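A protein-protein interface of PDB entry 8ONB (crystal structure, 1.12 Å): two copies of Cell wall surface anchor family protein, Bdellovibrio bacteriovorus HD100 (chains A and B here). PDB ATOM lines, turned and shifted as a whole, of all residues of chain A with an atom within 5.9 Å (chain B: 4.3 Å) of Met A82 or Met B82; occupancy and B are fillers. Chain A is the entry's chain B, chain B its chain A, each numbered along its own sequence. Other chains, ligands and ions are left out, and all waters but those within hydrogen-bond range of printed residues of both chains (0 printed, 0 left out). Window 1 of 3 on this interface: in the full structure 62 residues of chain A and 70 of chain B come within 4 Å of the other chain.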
ATOM      1  N   PRO A  68     -15.906  13.579  -5.203  1.00  0.00           N
ATOM      2  CA  PRO A  68     -14.613  14.269  -5.198  1.00  0.00           C
ATOM      3  C   PRO A  68     -14.615  15.318  -4.091  1.00  0.00           C
ATOM      4  O   PRO A  68     -15.567  16.103  -3.934  1.00  0.00           O
ATOM      5  CB  PRO A  68     -14.535  14.880  -6.602  1.00  0.00           C
ATOM      6  CG  PRO A  68     -15.994  15.138  -6.949  1.00  0.00           C
ATOM      7  CD  PRO A  68     -16.780  14.029  -6.308  1.00  0.00           C
ATOM      8  N   SER A  69     -13.537  15.321  -3.313  1.00  0.00           N
ATOM      9  CA  SER A  69     -13.477  16.041  -2.054  1.00  0.00           C
ATOM     10  C   SER A  69     -12.119  16.702  -1.882  1.00  0.00           C
ATOM     11  O   SER A  69     -11.076  16.152  -2.256  1.00  0.00           O
ATOM     12  CB  SER A  69     -13.714  15.095  -0.862  1.00  0.00           C
ATOM     13  OG  SER A  69     -14.967  14.427  -0.975  1.00  0.00           O
ATOM     14  N   LEU A  70     -12.158  17.882  -1.294  1.00  0.00           N
ATOM     15  CA  LEU A  70     -11.007  18.539  -0.698  1.00  0.00           C
ATOM     16  C   LEU A  70     -11.221  18.437   0.815  1.00  0.00           C
ATOM     17  O   LEU A  70     -12.220  18.953   1.340  1.00  0.00           O
ATOM     18  CB  LEU A  70     -10.948  19.993  -1.151  1.00  0.00           C
ATOM     19  CG  LEU A  70      -9.930  20.894  -0.446  1.00  0.00           C
ATOM     20  CD1 LEU A  70      -8.522  20.458  -0.852  1.00  0.00           C
ATOM     21  CD2 LEU A  70     -10.167  22.366  -0.755  1.00  0.00           C
ATOM     22  N   ILE A  71     -10.325  17.760   1.517  1.00  0.00           N
ATOM     23  CA  ILE A  71     -10.493  17.492   2.942  1.00  0.00           C
ATOM     24  C   ILE A  71      -9.351  18.169   3.680  1.00  0.00           C
ATOM     25  O   ILE A  71      -8.181  17.979   3.317  1.00  0.00           O
ATOM     26  CB  ILE A  71     -10.520  15.985   3.208  1.00  0.00           C
ATOM     27  CG1 ILE A  71     -11.655  15.335   2.418  1.00  0.00           C
ATOM     28  CG2 ILE A  71     -10.600  15.714   4.706  1.00  0.00           C
ATOM     29  CD1 ILE A  71     -11.467  13.822   2.194  1.00  0.00           C
ATOM     30  N   TYR A  72      -9.675  18.951   4.719  1.00  0.00           N
ATOM     31  CA  TYR A  72      -8.678  19.540   5.594  1.00  0.00           C
ATOM     32  C   TYR A  72      -8.649  18.792   6.916  1.00  0.00           C
ATOM     33  O   TYR A  72      -9.696  18.592   7.553  1.00  0.00           O
ATOM     34  CB  TYR A  72      -9.024  20.976   5.905  1.00  0.00           C
ATOM     35  CG  TYR A  72      -8.993  21.941   4.750  1.00  0.00           C
ATOM     36  CD1 TYR A  72     -10.091  22.103   3.914  1.00  0.00           C
ATOM     37  CD2 TYR A  72      -7.866  22.725   4.521  1.00  0.00           C
ATOM     38  CE1 TYR A  72     -10.063  23.031   2.871  1.00  0.00           C
ATOM     39  CE2 TYR A  72      -7.827  23.637   3.477  1.00  0.00           C
ATOM     40  CZ  TYR A  72      -8.922  23.799   2.666  1.00  0.00           C
ATOM     41  OH  TYR A  72      -8.954  24.719   1.653  1.00  0.00           O
ATOM     42  N   TRP A  80     -12.611  20.039   8.205  1.00  0.00           N
ATOM     43  CA  TRP A  80     -13.512  20.639   7.186  1.00  0.00           C
ATOM     44  C   TRP A  80     -13.328  19.933   5.846  1.00  0.00           C
ATOM     45  O   TRP A  80     -12.262  19.341   5.619  1.00  0.00           O
ATOM     46  CB  TRP A  80     -13.202  22.130   6.988  1.00  0.00           C
ATOM     47  CG  TRP A  80     -13.538  22.998   8.158  1.00  0.00           C
ATOM     48  CD1 TRP A  80     -12.725  23.314   9.208  1.00  0.00           C
ATOM     49  CD2 TRP A  80     -14.788  23.665   8.400  1.00  0.00           C
ATOM     50  NE1 TRP A  80     -13.385  24.123  10.092  1.00  0.00           N
ATOM     51  CE2 TRP A  80     -14.649  24.361   9.620  1.00  0.00           C
ATOM     52  CE3 TRP A  80     -16.000  23.746   7.706  1.00  0.00           C
ATOM     53  CZ2 TRP A  80     -15.682  25.124  10.158  1.00  0.00           C
ATOM     54  CZ3 TRP A  80     -17.019  24.504   8.237  1.00  0.00           C
ATOM     55  CH2 TRP A  80     -16.857  25.182   9.446  1.00  0.00           C
ATOM     56  N   SER A  81     -14.359  19.978   5.008  1.00  0.00           N
ATOM     57  CA  SER A  81     -14.217  19.437   3.637  1.00  0.00           C
ATOM     58  C   SER A  81     -15.122  20.227   2.693  1.00  0.00           C
ATOM     59  O   SER A  81     -16.112  20.819   3.165  1.00  0.00           O
ATOM     60  CB  SER A  81     -14.498  17.960   3.571  1.00  0.00           C
ATOM     61  OG  SER A  81     -15.882  17.710   3.737  1.00  0.00           O
ATOM     62  N   MET A  82     -14.689  20.390   1.501  1.00  0.00           N
ATOM     63  CA  MET A  82     -15.555  20.926   0.418  1.00  0.00           C
ATOM     64  C   MET A  82     -15.653  19.883  -0.702  1.00  0.00           C
ATOM     65  O   MET A  82     -14.586  19.462  -1.186  1.00  0.00           O
ATOM     66  CB  MET A  82     -14.989  22.235  -0.142  1.00  0.00           C
ATOM     67  CG  MET A  82     -15.865  22.852  -1.216  1.00  0.00           C
ATOM     68  SD  MET A  82     -15.447  24.575  -1.571  1.00  0.00           S
ATOM     69  CE  MET A  82     -13.949  24.362  -2.526  1.00  0.00           C
ATOM     70  N   MET A  83     -16.833  19.410  -0.881  1.00  0.00           N
ATOM     71  CA  MET A  83     -16.975  18.273  -1.812  1.00  0.00           C
ATOM     72  C   MET A  83     -18.263  18.341  -2.619  1.00  0.00           C
ATOM     73  O   MET A  83     -19.099  19.198  -2.370  1.00  0.00           O
ATOM     74  CB  MET A  83     -17.014  16.974  -1.005  1.00  0.00           C
ATOM     75  CG  MET A  83     -18.133  16.940   0.020  1.00  0.00           C
ATOM     76  SD  MET A  83     -18.611  15.278   0.606  1.00  0.00           S
ATOM     77  CE  MET A  83     -19.805  14.832  -0.647  1.00  0.00           C
ATOM     78  N   VAL A  84     -18.264  17.555  -3.693  1.00  0.00           N
ATOM     79  CA  VAL A  84     -19.450  17.437  -4.558  1.00  0.00           C
ATOM     80  C   VAL A  84     -20.156  16.167  -4.078  1.00  0.00           C
ATOM     81  O   VAL A  84     -19.554  15.081  -4.090  1.00  0.00           O
ATOM     82  CB  VAL A  84     -19.074  17.411  -6.042  1.00  0.00           C
ATOM     83  CG1 VAL A  84     -20.321  17.282  -6.882  1.00  0.00           C
ATOM     84  CG2 VAL A  84     -18.298  18.668  -6.419  1.00  0.00           C
ATOM     85  N   LEU A  98     -22.798  21.101  -4.158  1.00  0.00           N
ATOM     86  CA  LEU A  98     -21.558  21.377  -3.386  1.00  0.00           C
ATOM     87  C   LEU A  98     -21.905  21.485  -1.897  1.00  0.00           C
ATOM     88  O   LEU A  98     -22.809  22.278  -1.581  1.00  0.00           O
ATOM     89  CB  LEU A  98     -20.930  22.673  -3.907  1.00  0.00           C
ATOM     90  CG  LEU A  98     -19.504  22.943  -3.426  1.00  0.00           C
ATOM     91  CD1 LEU A  98     -18.524  21.974  -4.071  1.00  0.00           C
ATOM     92  CD2 LEU A  98     -19.099  24.378  -3.716  1.00  0.00           C
ATOM     93  N   SER A  99     -21.102  20.947  -1.108  1.00  0.00           N
ATOM     94  CA  SER A  99     -21.286  21.017   0.335  1.00  0.00           C
ATOM     95  C   SER A  99     -19.966  21.280   1.032  1.00  0.00           C
ATOM     96  O   SER A  99     -18.948  20.649   0.711  1.00  0.00           O
ATOM     97  CB  SER A  99     -21.859  19.721   0.897  1.00  0.00           C
ATOM     98  OG  SER A  99     -23.227  19.566   0.565  1.00  0.00           O
ATOM     99  N   ILE A 100     -20.007  22.194   1.999  1.00  0.00           N
ATOM    100  CA  ILE A 100     -18.897  22.436   2.910  1.00  0.00           C
ATOM    101  C   ILE A 100     -19.301  21.815   4.226  1.00  0.00           C
ATOM    102  O   ILE A 100     -20.293  22.250   4.849  1.00  0.00           O
ATOM    103  CB  ILE A 100     -18.576  23.925   3.073  1.00  0.00           C
ATOM    104  CG1 ILE A 100     -18.128  24.547   1.746  1.00  0.00           C
ATOM    105  CG2 ILE A 100     -17.500  24.105   4.147  1.00  0.00           C
ATOM    106  CD1 ILE A 100     -17.868  26.036   1.816  1.00  0.00           C
ATOM    107  N   LEU A 101     -18.593  20.760   4.609  1.00  0.00           N
ATOM    108  CA  LEU A 101     -18.861  20.005   5.818  1.00  0.00           C
ATOM    109  C   LEU A 101     -17.899  20.415   6.915  1.00  0.00           C
ATOM    110  O   LEU A 101     -16.723  20.686   6.663  1.00  0.00           O
ATOM    111  CB  LEU A 101     -18.681  18.501   5.587  1.00  0.00           C
ATOM    112  CG  LEU A 101     -19.412  17.911   4.385  1.00  0.00           C
ATOM    113  CD1 LEU A 101     -19.178  16.406   4.336  1.00  0.00           C
ATOM    114  CD2 LEU A 101     -20.872  18.164   4.523  1.00  0.00           C
ATOM    115  N   SER B  69      -3.721  24.690   4.279  1.00  0.00           N
ATOM    116  CA  SER B  69      -4.183  25.778   3.421  1.00  0.00           C
ATOM    117  C   SER B  69      -4.159  25.372   1.954  1.00  0.00           C
ATOM    118  O   SER B  69      -3.244  24.678   1.498  1.00  0.00           O
ATOM    119  CB  SER B  69      -3.295  26.996   3.556  1.00  0.00           C
ATOM    120  OG  SER B  69      -3.095  27.358   4.890  1.00  0.00           O
ATOM    121  N   LEU B  70      -5.157  25.824   1.211  1.00  0.00           N
ATOM    122  CA  LEU B  70      -5.162  25.853  -0.242  1.00  0.00           C
ATOM    123  C   LEU B  70      -4.952  27.307  -0.660  1.00  0.00           C
ATOM    124  O   LEU B  70      -5.727  28.185  -0.266  1.00  0.00           O
ATOM    125  CB  LEU B  70      -6.502  25.341  -0.744  1.00  0.00           C
ATOM    126  CG  LEU B  70      -6.660  25.438  -2.259  1.00  0.00           C
ATOM    127  CD1 LEU B  70      -5.649  24.541  -2.990  1.00  0.00           C
ATOM    128  CD2 LEU B  70      -8.085  25.097  -2.638  1.00  0.00           C
ATOM    129  N   SER B  81      -6.728  32.489  -0.238  1.00  0.00           N
ATOM    130  CA  SER B  81      -6.540  31.145   0.300  1.00  0.00           C
ATOM    131  C   SER B  81      -7.786  30.704   1.023  1.00  0.00           C
ATOM    132  O   SER B  81      -8.621  31.520   1.430  1.00  0.00           O
ATOM    133  CB  SER B  81      -5.348  31.080   1.241  1.00  0.00           C
ATOM    134  OG  SER B  81      -5.500  31.940   2.366  1.00  0.00           O
ATOM    135  N   MET B  82      -7.929  29.394   1.140  1.00  0.00           N
ATOM    136  CA  MET B  82      -8.973  28.780   2.003  1.00  0.00           C
ATOM    137  C   MET B  82      -8.207  27.860   2.962  1.00  0.00           C
ATOM    138  O   MET B  82      -7.520  26.954   2.515  1.00  0.00           O
ATOM    139  CB  MET B  82     -10.043  28.016   1.233  1.00  0.00           C
ATOM    140  CG  MET B  82     -11.082  27.449   2.174  1.00  0.00           C
ATOM    141  SD  MET B  82     -12.615  27.098   1.346  1.00  0.00           S
ATOM    142  CE  MET B  82     -12.179  25.523   0.672  1.00  0.00           C
ATOM    143  N   MET B  83      -8.355  28.132   4.247  1.00  0.00           N
ATOM    144  CA  MET B  83      -7.536  27.381   5.215  1.00  0.00           C
ATOM    145  C   MET B  83      -8.320  27.106   6.495  1.00  0.00           C
ATOM    146  O   MET B  83      -9.312  27.750   6.758  1.00  0.00           O
ATOM    147  CB  MET B  83      -6.305  28.207   5.610  1.00  0.00           C
ATOM    148  CG  MET B  83      -6.651  29.486   6.398  1.00  0.00           C
ATOM    149  SD  MET B  83      -5.147  30.313   7.069  1.00  0.00           S
ATOM    150  CE  MET B  83      -4.379  30.811   5.545  1.00  0.00           C
ATOM    151  N   LEU B  98     -12.952  27.556   9.537  1.00  0.00           N
ATOM    152  CA  LEU B  98     -12.592  27.655   8.130  1.00  0.00           C
ATOM    153  C   LEU B  98     -12.565  29.117   7.733  1.00  0.00           C
ATOM    154  O   LEU B  98     -13.524  29.830   8.015  1.00  0.00           O
ATOM    155  CB  LEU B  98     -13.622  26.945   7.254  1.00  0.00           C
ATOM    156  CG  LEU B  98     -13.218  26.796   5.779  1.00  0.00           C
ATOM    157  CD1 LEU B  98     -12.026  25.858   5.620  1.00  0.00           C
ATOM    158  CD2 LEU B  98     -14.394  26.235   4.994  1.00  0.00           C
ATOM    159  N   SER B  99     -11.472  29.562   7.116  1.00  0.00           N
ATOM    160  CA  SER B  99     -11.364  30.984   6.723  1.00  0.00           C
ATOM    161  C   SER B  99     -10.963  31.079   5.253  1.00  0.00           C
ATOM    162  O   SER B  99     -10.151  30.282   4.782  1.00  0.00           O
ATOM    163  CB  SER B  99     -10.345  31.733   7.566  1.00  0.00           C
ATOM    164  OG  SER B  99     -10.842  32.047   8.862  1.00  0.00           O
ATOM    165  N   ILE B 100     -11.557  32.046   4.579  1.00  0.00           N
ATOM    166  CA  ILE B 100     -11.148  32.425   3.236  1.00  0.00           C
ATOM    167  C   ILE B 100     -10.503  33.798   3.347  1.00  0.00           C
ATOM    168  O   ILE B 100     -11.173  34.763   3.767  1.00  0.00           O
ATOM    169  CB  ILE B 100     -12.323  32.457   2.254  1.00  0.00           C
ATOM    170  CG1 ILE B 100     -13.025  31.105   2.206  1.00  0.00           C
ATOM    171  CG2 ILE B 100     -11.864  32.985   0.901  1.00  0.00           C
ATOM    172  CD1 ILE B 100     -14.239  31.056   1.316  1.00  0.00           C
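Of the 8 printed residues of chain B, 3 touch a printed residue of chain A. Of the 14 printed residues of chain A, 5 touch a printed residue of chain B. Printed residues of chain A that touch a printed residue of chain B: Leu A70, Tyr A72, Trp A80, Met A82 and Ile A100. Among the printed residues, 6 pairs touch across the chains. Among the printed residues, no Asp or Glu carboxylate lies within 4 Å of a Lys or Arg side-chain nitrogen of the other chain.
Leu A70 touches Leu B70 (CD2 to CD2, 3.9 Å). Leu B70 touches Tyr A72. Trp A80 touches Leu B98. Met B82 touches Met A82. Leu B98 touches Ile A100.
The backbone carbonyl oxygen (O) of Leu B70 is in hydrogen-bond range of the backbone NH (N) of Met B82 (2.9 Å). The backbone carbonyl oxygen (O) of Leu A70 is in hydrogen-bond range of the backbone NH (N) of Met A82. O of Trp A80 sits at hydrogen-bond distance from N of Tyr A72 (2.8 Å).
Leu B70 touches its own counterpart, Leu A70. Met B82 touches its own counterpart, Met A82. Ile A100 touches Leu B98, but with the chains exchanged Leu A98 does not touch Ile B100 (9.7 Å). 8 positions are printed for both chains.
Met A82 touches just one residue of chain B: Met B82 (3.8 Å). Printed residues of chain A within 4 Å of Met B82: Tyr A72 and Met A82. Of the printed residues of chain A, Leu B70 touches Leu A70 and Tyr A72. Of the printed residues of chain A, Leu B98 touches Trp A80 and Ile A100. Of the printed residues of chain B, Ile A100 touches Leu B98. Printed residues of chain B within 4 Å of Leu A70: Leu B70. The nearest printed residue of chain A that does not touch Met B82 is Leu A70 (4.01 Å). The nearest printed residue of chain A that does not touch Leu B70 is Met A82 (5.9 Å).
The backbone carbonyl oxygen (O) of Met B82 sits at hydrogen-bond distance from the side-chain hydroxyl (OH) of Tyr A72 (2.8 Å).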
